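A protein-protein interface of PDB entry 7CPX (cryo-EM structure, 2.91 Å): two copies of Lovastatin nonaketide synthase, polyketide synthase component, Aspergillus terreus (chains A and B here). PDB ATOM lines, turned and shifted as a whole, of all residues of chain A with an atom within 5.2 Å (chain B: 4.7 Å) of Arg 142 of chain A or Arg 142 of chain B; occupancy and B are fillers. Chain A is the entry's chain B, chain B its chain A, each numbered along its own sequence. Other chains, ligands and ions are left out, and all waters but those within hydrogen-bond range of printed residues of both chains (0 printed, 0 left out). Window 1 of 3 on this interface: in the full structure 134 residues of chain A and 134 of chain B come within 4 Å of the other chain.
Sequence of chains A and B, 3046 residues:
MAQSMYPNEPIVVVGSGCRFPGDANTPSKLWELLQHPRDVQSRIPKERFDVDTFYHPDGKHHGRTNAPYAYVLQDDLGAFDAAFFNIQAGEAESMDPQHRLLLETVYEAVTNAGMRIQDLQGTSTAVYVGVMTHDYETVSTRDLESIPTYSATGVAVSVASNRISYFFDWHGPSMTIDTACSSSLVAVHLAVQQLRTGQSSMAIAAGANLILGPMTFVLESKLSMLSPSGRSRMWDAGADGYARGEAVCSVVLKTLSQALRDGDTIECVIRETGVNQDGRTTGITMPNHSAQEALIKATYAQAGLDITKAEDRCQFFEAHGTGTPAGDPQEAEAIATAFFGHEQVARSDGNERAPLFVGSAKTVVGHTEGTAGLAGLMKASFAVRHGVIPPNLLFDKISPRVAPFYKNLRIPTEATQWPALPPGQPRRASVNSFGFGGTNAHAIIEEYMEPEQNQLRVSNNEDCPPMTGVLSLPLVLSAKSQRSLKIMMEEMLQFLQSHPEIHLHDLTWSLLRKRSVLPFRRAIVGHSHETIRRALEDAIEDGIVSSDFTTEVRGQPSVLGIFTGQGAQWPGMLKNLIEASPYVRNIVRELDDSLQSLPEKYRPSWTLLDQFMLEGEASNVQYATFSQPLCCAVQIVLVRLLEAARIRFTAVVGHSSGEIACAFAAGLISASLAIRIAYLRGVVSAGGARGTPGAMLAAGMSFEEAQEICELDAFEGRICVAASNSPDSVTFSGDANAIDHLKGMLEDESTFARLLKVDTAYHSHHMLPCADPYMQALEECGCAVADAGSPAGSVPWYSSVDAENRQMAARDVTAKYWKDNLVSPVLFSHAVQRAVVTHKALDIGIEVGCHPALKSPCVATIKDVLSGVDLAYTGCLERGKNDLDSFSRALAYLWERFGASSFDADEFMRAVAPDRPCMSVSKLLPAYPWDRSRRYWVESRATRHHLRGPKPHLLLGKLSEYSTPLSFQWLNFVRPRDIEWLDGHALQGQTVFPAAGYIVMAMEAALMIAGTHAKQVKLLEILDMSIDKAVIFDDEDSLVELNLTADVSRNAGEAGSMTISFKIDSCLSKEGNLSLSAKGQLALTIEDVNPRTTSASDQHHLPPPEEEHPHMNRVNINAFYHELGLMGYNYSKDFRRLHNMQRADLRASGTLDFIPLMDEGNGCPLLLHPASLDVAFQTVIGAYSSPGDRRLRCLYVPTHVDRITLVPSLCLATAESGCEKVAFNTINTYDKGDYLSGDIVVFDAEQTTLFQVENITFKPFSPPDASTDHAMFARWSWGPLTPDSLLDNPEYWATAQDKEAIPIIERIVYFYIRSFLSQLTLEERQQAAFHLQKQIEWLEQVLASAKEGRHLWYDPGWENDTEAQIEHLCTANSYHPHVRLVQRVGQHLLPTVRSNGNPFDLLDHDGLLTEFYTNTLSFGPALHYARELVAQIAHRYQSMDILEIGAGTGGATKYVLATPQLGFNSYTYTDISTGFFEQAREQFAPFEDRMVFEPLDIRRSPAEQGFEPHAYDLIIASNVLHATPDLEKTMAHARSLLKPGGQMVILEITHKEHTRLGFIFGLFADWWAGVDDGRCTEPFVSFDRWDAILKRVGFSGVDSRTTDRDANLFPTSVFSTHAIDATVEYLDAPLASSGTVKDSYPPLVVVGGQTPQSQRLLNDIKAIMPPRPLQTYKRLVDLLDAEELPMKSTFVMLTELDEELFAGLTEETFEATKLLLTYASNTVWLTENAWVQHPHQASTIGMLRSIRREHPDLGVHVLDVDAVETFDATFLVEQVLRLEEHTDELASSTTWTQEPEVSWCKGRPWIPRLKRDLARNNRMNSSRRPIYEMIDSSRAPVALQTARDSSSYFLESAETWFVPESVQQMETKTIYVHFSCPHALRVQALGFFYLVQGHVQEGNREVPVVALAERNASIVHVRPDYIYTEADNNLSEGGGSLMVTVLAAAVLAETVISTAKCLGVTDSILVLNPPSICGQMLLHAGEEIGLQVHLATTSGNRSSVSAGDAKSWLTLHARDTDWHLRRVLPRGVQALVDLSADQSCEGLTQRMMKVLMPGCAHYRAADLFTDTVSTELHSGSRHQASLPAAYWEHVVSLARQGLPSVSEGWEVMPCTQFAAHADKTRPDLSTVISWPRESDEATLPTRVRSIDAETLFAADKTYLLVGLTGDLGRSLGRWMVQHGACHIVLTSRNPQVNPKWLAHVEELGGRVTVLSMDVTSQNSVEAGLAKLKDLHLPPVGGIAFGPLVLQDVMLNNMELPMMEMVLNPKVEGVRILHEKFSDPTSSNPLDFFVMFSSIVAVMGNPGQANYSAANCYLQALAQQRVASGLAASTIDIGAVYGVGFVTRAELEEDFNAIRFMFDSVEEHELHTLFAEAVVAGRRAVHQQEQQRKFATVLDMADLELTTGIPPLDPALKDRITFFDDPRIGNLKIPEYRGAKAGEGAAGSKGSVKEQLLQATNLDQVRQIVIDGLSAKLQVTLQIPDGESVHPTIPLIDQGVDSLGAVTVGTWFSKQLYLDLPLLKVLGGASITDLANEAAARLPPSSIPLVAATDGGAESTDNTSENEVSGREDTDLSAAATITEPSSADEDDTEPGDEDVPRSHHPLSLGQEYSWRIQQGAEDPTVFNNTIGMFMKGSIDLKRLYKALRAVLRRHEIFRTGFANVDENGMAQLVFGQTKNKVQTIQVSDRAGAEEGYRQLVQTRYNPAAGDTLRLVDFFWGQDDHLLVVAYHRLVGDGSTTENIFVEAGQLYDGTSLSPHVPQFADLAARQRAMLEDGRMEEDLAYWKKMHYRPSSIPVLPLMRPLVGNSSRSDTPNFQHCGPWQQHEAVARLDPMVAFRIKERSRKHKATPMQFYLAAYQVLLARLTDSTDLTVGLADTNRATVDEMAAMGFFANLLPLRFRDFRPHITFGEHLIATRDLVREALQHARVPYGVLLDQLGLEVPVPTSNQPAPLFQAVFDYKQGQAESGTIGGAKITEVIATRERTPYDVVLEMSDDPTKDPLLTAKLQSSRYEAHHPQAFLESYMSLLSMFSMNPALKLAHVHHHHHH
O of Arg 142 of chain B sits at hydrogen-bond distance from NE of Arg 142 of chain A, 3.5 Å away.
The side-chain hydroxyl (OG1) of Thr 141 of chain B sits close to the backbone NH (N) of Thr 138 of chain B (3.4 Å).
OD1 of Asp 143 of chain B lies within salt-bridge range of NH1 of Arg 142 of chain B (3.8 Å).
NE of Arg 142 of chain B is in hydrogen-bond range of NE2 of His 946 of chain B (3.4 Å).
The backbone NH (N) of Thr 138 of chain A sits close to the side-chain hydroxyl (OG1) of Thr 141 of chain A, at 3.4 Å.
The guanidinium group (NH1) of Arg 142 of chain A lies within salt-bridge range of the side-chain carboxylate (OD1) of Asp 143 of chain A (3.9 Å).
NH2 of Arg 142 of chain A is in salt-bridge range of OE2 of Glu 961 of chain A (2.7 Å).
Among the printed residues, merely in contact across the chains: Thr 141 of chain A with Met 215 of chain B (2.9 Å), Met 215 of chain A with Thr 141 of chain B (2.9 Å), His 946 of chain A with Leu 144 of chain B (3.4 Å), Leu 144 of chain A with His 946 of chain B (3.4 Å), Leu 144 of chain A with Met 215 of chain B (3.7 Å) and Met 215 of chain A with Leu 144 of chain B (3.7 Å).
Printed residues of chain B within 4 Å of Thr 141 of chain A: Met 215 (2.9 Å).
Arg 142 of chain A touches just one residue of chain B: Arg 142 (3.5 Å).
Of chain A, only Arg 142 (3.5 Å) comes within 4 Å of Arg 142 of chain B.
Printed residues of chain A within 4 Å of Leu 144 of chain B: Met 215 and His 946.
Thr 943 of chain B touches none of the printed residues of chain A.
The nearest residue of chain B that does not touch Arg 142 of chain A is Met 215 of chain B (4.5 Å).
The nearest printed residue of chain A that does not touch His 946 of chain B is Arg 142 of chain A (6.0 Å).
Along chain B the printed residues that touch a printed residue of chain A span positions 141 to 946.
Among the printed residues, no Asp or Glu carboxylate lies within 4 Å of a Lys or Arg side-chain nitrogen of the other chain.
Thr 141 of chain A touches Met 215 of chain B, and with the chains exchanged Met 215 of chain A touches Thr 141 of chain B.
Arg 142 of chain A touches its own counterpart, Arg 142 of chain B.
Leu 144 of chain A touches Met 215 of chain B, and with the chains exchanged Met 215 of chain A touches Leu 144 of chain B.
Leu 144 of chain A touches His 946 of chain B, and with the chains exchanged His 946 of chain A touches Leu 144 of chain B.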
ATOM      1  N   THR A 138     -30.427  30.830  23.135  1.00  0.00           N
ATOM      2  CA  THR A 138     -30.507  29.415  23.468  1.00  0.00           C
ATOM      3  C   THR A 138     -30.862  28.575  22.254  1.00  0.00           C
ATOM      4  O   THR A 138     -30.156  27.609  21.944  1.00  0.00           O
ATOM      5  CB  THR A 138     -31.539  29.189  24.580  1.00  0.00           C
ATOM      6  OG1 THR A 138     -31.228  30.021  25.704  1.00  0.00           O
ATOM      7  CG2 THR A 138     -31.531  27.739  25.012  1.00  0.00           C
ATOM      8  N   VAL A 139     -31.938  28.927  21.549  1.00  0.00           N
ATOM      9  CA  VAL A 139     -32.287  28.228  20.317  1.00  0.00           C
ATOM     10  C   VAL A 139     -31.156  28.352  19.305  1.00  0.00           C
ATOM     11  O   VAL A 139     -30.693  27.357  18.736  1.00  0.00           O
ATOM     12  CB  VAL A 139     -33.607  28.779  19.751  1.00  0.00           C
ATOM     13  CG1 VAL A 139     -33.809  28.313  18.323  1.00  0.00           C
ATOM     14  CG2 VAL A 139     -34.764  28.350  20.624  1.00  0.00           C
ATOM     15  N   SER A 140     -30.692  29.579  19.071  1.00  0.00           N
ATOM     16  CA  SER A 140     -29.608  29.805  18.128  1.00  0.00           C
ATOM     17  C   SER A 140     -28.259  29.352  18.665  1.00  0.00           C
ATOM     18  O   SER A 140     -27.294  29.303  17.896  1.00  0.00           O
ATOM     19  CB  SER A 140     -29.538  31.287  17.762  1.00  0.00           C
ATOM     20  OG  SER A 140     -28.464  31.545  16.875  1.00  0.00           O
ATOM     21  N   THR A 141     -28.168  29.027  19.953  1.00  0.00           N
ATOM     22  CA  THR A 141     -26.908  28.632  20.558  1.00  0.00           C
ATOM     23  C   THR A 141     -26.977  27.293  21.277  1.00  0.00           C
ATOM     24  O   THR A 141     -25.975  26.882  21.871  1.00  0.00           O
ATOM     25  CB  THR A 141     -26.429  29.706  21.546  1.00  0.00           C
ATOM     26  OG1 THR A 141     -27.254  29.688  22.719  1.00  0.00           O
ATOM     27  CG2 THR A 141     -26.500  31.082  20.907  1.00  0.00           C
ATOM     28  N   ARG A 142     -28.117  26.601  21.243  1.00  0.00           N
ATOM     29  CA  ARG A 142     -28.191  25.290  21.877  1.00  0.00           C
ATOM     30  C   ARG A 142     -27.129  24.364  21.304  1.00  0.00           C
ATOM     31  O   ARG A 142     -26.440  23.651  22.043  1.00  0.00           O
ATOM     32  CB  ARG A 142     -29.583  24.687  21.693  1.00  0.00           C
ATOM     33  CG  ARG A 142     -30.134  24.046  22.952  1.00  0.00           C
ATOM     34  CD  ARG A 142     -31.455  23.344  22.696  1.00  0.00           C
ATOM     35  NE  ARG A 142     -31.488  22.029  23.323  1.00  0.00           N
ATOM     36  CZ  ARG A 142     -31.013  20.924  22.766  1.00  0.00           C
ATOM     37  NH1 ARG A 142     -30.470  20.935  21.559  1.00  0.00           N
ATOM     38  NH2 ARG A 142     -31.080  19.777  23.437  1.00  0.00           N
ATOM     39  N   ASP A 143     -26.979  24.368  19.983  1.00  0.00           N
ATOM     40  CA  ASP A 143     -25.876  23.690  19.315  1.00  0.00           C
ATOM     41  C   ASP A 143     -24.792  24.726  19.050  1.00  0.00           C
ATOM     42  O   ASP A 143     -24.945  25.585  18.177  1.00  0.00           O
ATOM     43  CB  ASP A 143     -26.344  23.035  18.019  1.00  0.00           C
ATOM     44  CG  ASP A 143     -27.415  21.988  18.251  1.00  0.00           C
ATOM     45  OD1 ASP A 143     -28.570  22.369  18.533  1.00  0.00           O
ATOM     46  OD2 ASP A 143     -27.101  20.783  18.152  1.00  0.00           O
ATOM     47  N   LEU A 144     -23.698  24.651  19.812  1.00  0.00           N
ATOM     48  CA  LEU A 144     -22.636  25.638  19.664  1.00  0.00           C
ATOM     49  C   LEU A 144     -22.092  25.661  18.246  1.00  0.00           C
ATOM     50  O   LEU A 144     -21.695  26.720  17.749  1.00  0.00           O
ATOM     51  CB  LEU A 144     -21.520  25.352  20.662  1.00  0.00           C
ATOM     52  CG  LEU A 144     -21.907  25.680  22.102  1.00  0.00           C
ATOM     53  CD1 LEU A 144     -21.062  24.888  23.066  1.00  0.00           C
ATOM     54  CD2 LEU A 144     -21.757  27.165  22.364  1.00  0.00           C
ATOM     55  N   MET A 215     -37.622  26.314  26.174  1.00  0.00           N
ATOM     56  CA  MET A 215     -36.900  26.573  27.415  1.00  0.00           C
ATOM     57  C   MET A 215     -37.787  27.268  28.439  1.00  0.00           C
ATOM     58  O   MET A 215     -37.979  26.775  29.556  1.00  0.00           O
ATOM     59  CB  MET A 215     -35.660  27.432  27.134  1.00  0.00           C
ATOM     60  CG  MET A 215     -34.763  27.054  25.961  1.00  0.00           C
ATOM     61  SD  MET A 215     -33.904  25.482  26.171  1.00  0.00           S
ATOM     62  CE  MET A 215     -32.874  25.834  27.593  1.00  0.00           C
ATOM     63  N   ALA A 942     -29.913  20.041  14.057  1.00  0.00           N
ATOM     64  CA  ALA A 942     -30.163  19.452  15.366  1.00  0.00           C
ATOM     65  C   ALA A 942     -31.139  20.304  16.164  1.00  0.00           C
ATOM     66  O   ALA A 942     -32.069  19.781  16.789  1.00  0.00           O
ATOM     67  CB  ALA A 942     -28.846  19.292  16.124  1.00  0.00           C
ATOM     68  N   THR A 943     -30.953  21.625  16.143  1.00  0.00           N
ATOM     69  CA  THR A 943     -31.883  22.508  16.837  1.00  0.00           C
ATOM     70  C   THR A 943     -33.275  22.424  16.227  1.00  0.00           C
ATOM     71  O   THR A 943     -34.280  22.455  16.946  1.00  0.00           O
ATOM     72  CB  THR A 943     -31.372  23.947  16.802  1.00  0.00           C
ATOM     73  OG1 THR A 943     -30.138  24.038  17.525  1.00  0.00           O
ATOM     74  CG2 THR A 943     -32.388  24.883  17.426  1.00  0.00           C
ATOM     75  N   HIS A 946     -34.889  19.476  17.347  1.00  0.00           N
ATOM     76  CA  HIS A 946     -35.207  19.630  18.760  1.00  0.00           C
ATOM     77  C   HIS A 946     -36.518  20.383  18.955  1.00  0.00           C
ATOM     78  O   HIS A 946     -37.432  19.892  19.625  1.00  0.00           O
ATOM     79  CB  HIS A 946     -34.058  20.354  19.463  1.00  0.00           C
ATOM     80  CG  HIS A 946     -34.430  20.947  20.784  1.00  0.00           C
ATOM     81  ND1 HIS A 946     -34.917  20.192  21.828  1.00  0.00           N
ATOM     82  CD2 HIS A 946     -34.379  22.222  21.233  1.00  0.00           C
ATOM     83  CE1 HIS A 946     -35.154  20.977  22.863  1.00  0.00           C
ATOM     84  NE2 HIS A 946     -34.836  22.214  22.528  1.00  0.00           N
ATOM     85  N   GLU A 961     -31.431  14.844  18.705  1.00  0.00           N
ATOM     86  CA  GLU A 961     -31.361  15.843  17.647  1.00  0.00           C
ATOM     87  C   GLU A 961     -30.492  15.370  16.493  1.00  0.00           C
ATOM     88  O   GLU A 961     -30.749  15.719  15.336  1.00  0.00           O
ATOM     89  CB  GLU A 961     -30.815  17.161  18.197  1.00  0.00           C
ATOM     90  CG  GLU A 961     -31.560  17.718  19.400  1.00  0.00           C
ATOM     91  CD  GLU A 961     -31.069  17.154  20.719  1.00  0.00           C
ATOM     92  OE1 GLU A 961     -30.297  16.172  20.696  1.00  0.00           O
ATOM     93  OE2 GLU A 961     -31.455  17.691  21.778  1.00  0.00           O
ATOM     94  N   TYR A 962     -29.461  14.579  16.786  1.00  0.00           N
ATOM     95  CA  TYR A 962     -28.497  14.128  15.792  1.00  0.00           C
ATOM     96  C   TYR A 962     -28.821  12.736  15.268  1.00  0.00           C
ATOM     97  O   TYR A 962     -27.919  11.999  14.854  1.00  0.00           O
ATOM     98  CB  TYR A 962     -27.090  14.168  16.386  1.00  0.00           C
ATOM     99  CG  TYR A 962     -26.782  15.477  17.074  1.00  0.00           C
ATOM    100  CD1 TYR A 962     -26.272  16.554  16.367  1.00  0.00           C
ATOM    101  CD2 TYR A 962     -27.017  15.639  18.431  1.00  0.00           C
ATOM    102  CE1 TYR A 962     -25.997  17.751  16.992  1.00  0.00           C
ATOM    103  CE2 TYR A 962     -26.745  16.832  19.064  1.00  0.00           C
ATOM    104  CZ  TYR A 962     -26.236  17.887  18.339  1.00  0.00           C
ATOM    105  OH  TYR A 962     -25.961  19.080  18.967  1.00  0.00           O
ATOM    106  N   THR B 138     -28.432  28.228  30.761  1.00  0.00           N
ATOM    107  CA  THR B 138     -28.038  27.447  29.598  1.00  0.00           C
ATOM    108  C   THR B 138     -27.378  26.142  30.000  1.00  0.00           C
ATOM    109  O   THR B 138     -27.794  25.072  29.542  1.00  0.00           O
ATOM    110  CB  THR B 138     -27.090  28.260  28.707  1.00  0.00           C
ATOM    111  OG1 THR B 138     -27.699  29.512  28.371  1.00  0.00           O
ATOM    112  CG2 THR B 138     -26.781  27.496  27.439  1.00  0.00           C
ATOM    113  N   VAL B 139     -26.361  26.201  30.861  1.00  0.00           N
ATOM    114  CA  VAL B 139     -25.738  24.982  31.370  1.00  0.00           C
ATOM    115  C   VAL B 139     -26.766  24.137  32.108  1.00  0.00           C
ATOM    116  O   VAL B 139     -26.917  22.938  31.848  1.00  0.00           O
ATOM    117  CB  VAL B 139     -24.547  25.335  32.278  1.00  0.00           C
ATOM    118  CG1 VAL B 139     -24.106  24.121  33.071  1.00  0.00           C
ATOM    119  CG2 VAL B 139     -23.406  25.878  31.446  1.00  0.00           C
ATOM    120  N   SER B 140     -27.494  24.753  33.038  1.00  0.00           N
ATOM    121  CA  SER B 140     -28.508  24.037  33.797  1.00  0.00           C
ATOM    122  C   SER B 140     -29.748  23.730  32.973  1.00  0.00           C
ATOM    123  O   SER B 140     -30.597  22.958  33.431  1.00  0.00           O
ATOM    124  CB  SER B 140     -28.905  24.848  35.029  1.00  0.00           C
ATOM    125  OG  SER B 140     -29.923  24.195  35.766  1.00  0.00           O
ATOM    126  N   THR B 141     -29.875  24.312  31.780  1.00  0.00           N
ATOM    127  CA  THR B 141     -31.050  24.111  30.951  1.00  0.00           C
ATOM    128  C   THR B 141     -30.721  23.633  29.544  1.00  0.00           C
ATOM    129  O   THR B 141     -31.643  23.476  28.736  1.00  0.00           O
ATOM    130  CB  THR B 141     -31.867  25.408  30.858  1.00  0.00           C
ATOM    131  OG1 THR B 141     -31.176  26.359  30.038  1.00  0.00           O
ATOM    132  CG2 THR B 141     -32.078  26.000  32.240  1.00  0.00           C
ATOM    133  N   ARG B 142     -29.448  23.392  29.226  1.00  0.00           N
ATOM    134  CA  ARG B 142     -29.114  22.877  27.903  1.00  0.00           C
ATOM    135  C   ARG B 142     -29.859  21.578  27.635  1.00  0.00           C
ATOM    136  O   ARG B 142     -30.417  21.377  26.550  1.00  0.00           O
ATOM    137  CB  ARG B 142     -27.605  22.667  27.780  1.00  0.00           C
ATOM    138  CG  ARG B 142     -27.033  23.157  26.464  1.00  0.00           C
ATOM    139  CD  ARG B 142     -25.564  22.810  26.324  1.00  0.00           C
ATOM    140  NE  ARG B 142     -25.266  22.279  24.999  1.00  0.00           N
ATOM    141  CZ  ARG B 142     -25.402  21.005  24.658  1.00  0.00           C
ATOM    142  NH1 ARG B 142     -25.817  20.096  25.525  1.00  0.00           N
ATOM    143  NH2 ARG B 142     -25.118  20.632  23.414  1.00  0.00           N
ATOM    144  N   ASP B 143     -29.882  20.687  28.621  1.00  0.00           N
ATOM    145  CA  ASP B 143     -30.719  19.494  28.582  1.00  0.00           C
ATOM    146  C   ASP B 143     -31.995  19.801  29.354  1.00  0.00           C
ATOM    147  O   ASP B 143     -31.978  19.890  30.585  1.00  0.00           O
ATOM    148  CB  ASP B 143     -29.985  18.295  29.177  1.00  0.00           C
ATOM    149  CG  ASP B 143     -28.717  17.955  28.422  1.00  0.00           C
ATOM    150  OD1 ASP B 143     -27.722  18.697  28.564  1.00  0.00           O
ATOM    151  OD2 ASP B 143     -28.715  16.947  27.685  1.00  0.00           O
ATOM    152  N   LEU B 144     -33.102  19.973  28.629  1.00  0.00           N
ATOM    153  CA  LEU B 144     -34.355  20.327  29.283  1.00  0.00           C
ATOM    154  C   LEU B 144     -34.754  19.288  30.318  1.00  0.00           C
ATOM    155  O   LEU B 144     -35.352  19.632  31.344  1.00  0.00           O
ATOM    156  CB  LEU B 144     -35.455  20.497  28.241  1.00  0.00           C
ATOM    157  CG  LEU B 144     -35.295  21.763  27.403  1.00  0.00           C
ATOM    158  CD1 LEU B 144     -36.006  21.612  26.083  1.00  0.00           C
ATOM    159  CD2 LEU B 144     -35.828  22.965  28.155  1.00  0.00           C
ATOM    160  N   MET B 215     -20.662  28.719  26.202  1.00  0.00           N
ATOM    161  CA  MET B 215     -21.538  29.535  25.368  1.00  0.00           C
ATOM    162  C   MET B 215     -20.946  30.917  25.127  1.00  0.00           C
ATOM    163  O   MET B 215     -20.744  31.337  23.983  1.00  0.00           O
ATOM    164  CB  MET B 215     -22.918  29.667  26.021  1.00  0.00           C
ATOM    165  CG  MET B 215     -23.583  28.413  26.578  1.00  0.00           C
ATOM    166  SD  MET B 215     -24.046  27.206  25.318  1.00  0.00           S
ATOM    167  CE  MET B 215     -25.257  28.131  24.378  1.00  0.00           C
ATOM    168  N   THR B 943     -25.020  17.193  30.105  1.00  0.00           N
ATOM    169  CA  THR B 943     -24.402  18.508  30.241  1.00  0.00           C
ATOM    170  C   THR B 943     -22.982  18.391  30.776  1.00  0.00           C
ATOM    171  O   THR B 943     -22.087  19.129  30.348  1.00  0.00           O
ATOM    172  CB  THR B 943     -25.245  19.395  31.155  1.00  0.00           C
ATOM    173  OG1 THR B 943     -26.526  19.628  30.554  1.00  0.00           O
ATOM    174  CG2 THR B 943     -24.552  20.722  31.386  1.00  0.00           C
ATOM    175  N   HIS B 946     -20.804  17.393  28.167  1.00  0.00           N
ATOM    176  CA  HIS B 946     -20.666  18.501  27.229  1.00  0.00           C
ATOM    177  C   HIS B 946     -19.604  19.490  27.694  1.00  0.00           C
ATOM    178  O   HIS B 946     -18.663  19.798  26.953  1.00  0.00           O
ATOM    179  CB  HIS B 946     -22.018  19.196  27.062  1.00  0.00           C
ATOM    180  CG  HIS B 946     -21.927  20.572  26.486  1.00  0.00           C
ATOM    181  ND1 HIS B 946     -21.367  20.827  25.253  1.00  0.00           N
ATOM    182  CD2 HIS B 946     -22.331  21.770  26.971  1.00  0.00           C
ATOM    183  CE1 HIS B 946     -21.428  22.122  25.004  1.00  0.00           C
ATOM    184  NE2 HIS B 946     -22.007  22.717  26.031  1.00  0.00           N
ATOM    185  N   GLU B 961     -23.130  14.095  23.811  1.00  0.00           N
ATOM    186  CA  GLU B 961     -23.345  14.110  25.252  1.00  0.00           C
ATOM    187  C   GLU B 961     -23.962  12.807  25.735  1.00  0.00           C
ATOM    188  O   GLU B 961     -23.692  12.369  26.859  1.00  0.00           O
ATOM    189  CB  GLU B 961     -24.247  15.281  25.642  1.00  0.00           C
ATOM    190  CG  GLU B 961     -23.776  16.646  25.166  1.00  0.00           C
ATOM    191  CD  GLU B 961     -24.233  16.977  23.758  1.00  0.00           C
ATOM    192  OE1 GLU B 961     -24.736  16.067  23.066  1.00  0.00           O
ATOM    193  OE2 GLU B 961     -24.091  18.147  23.345  1.00  0.00           O
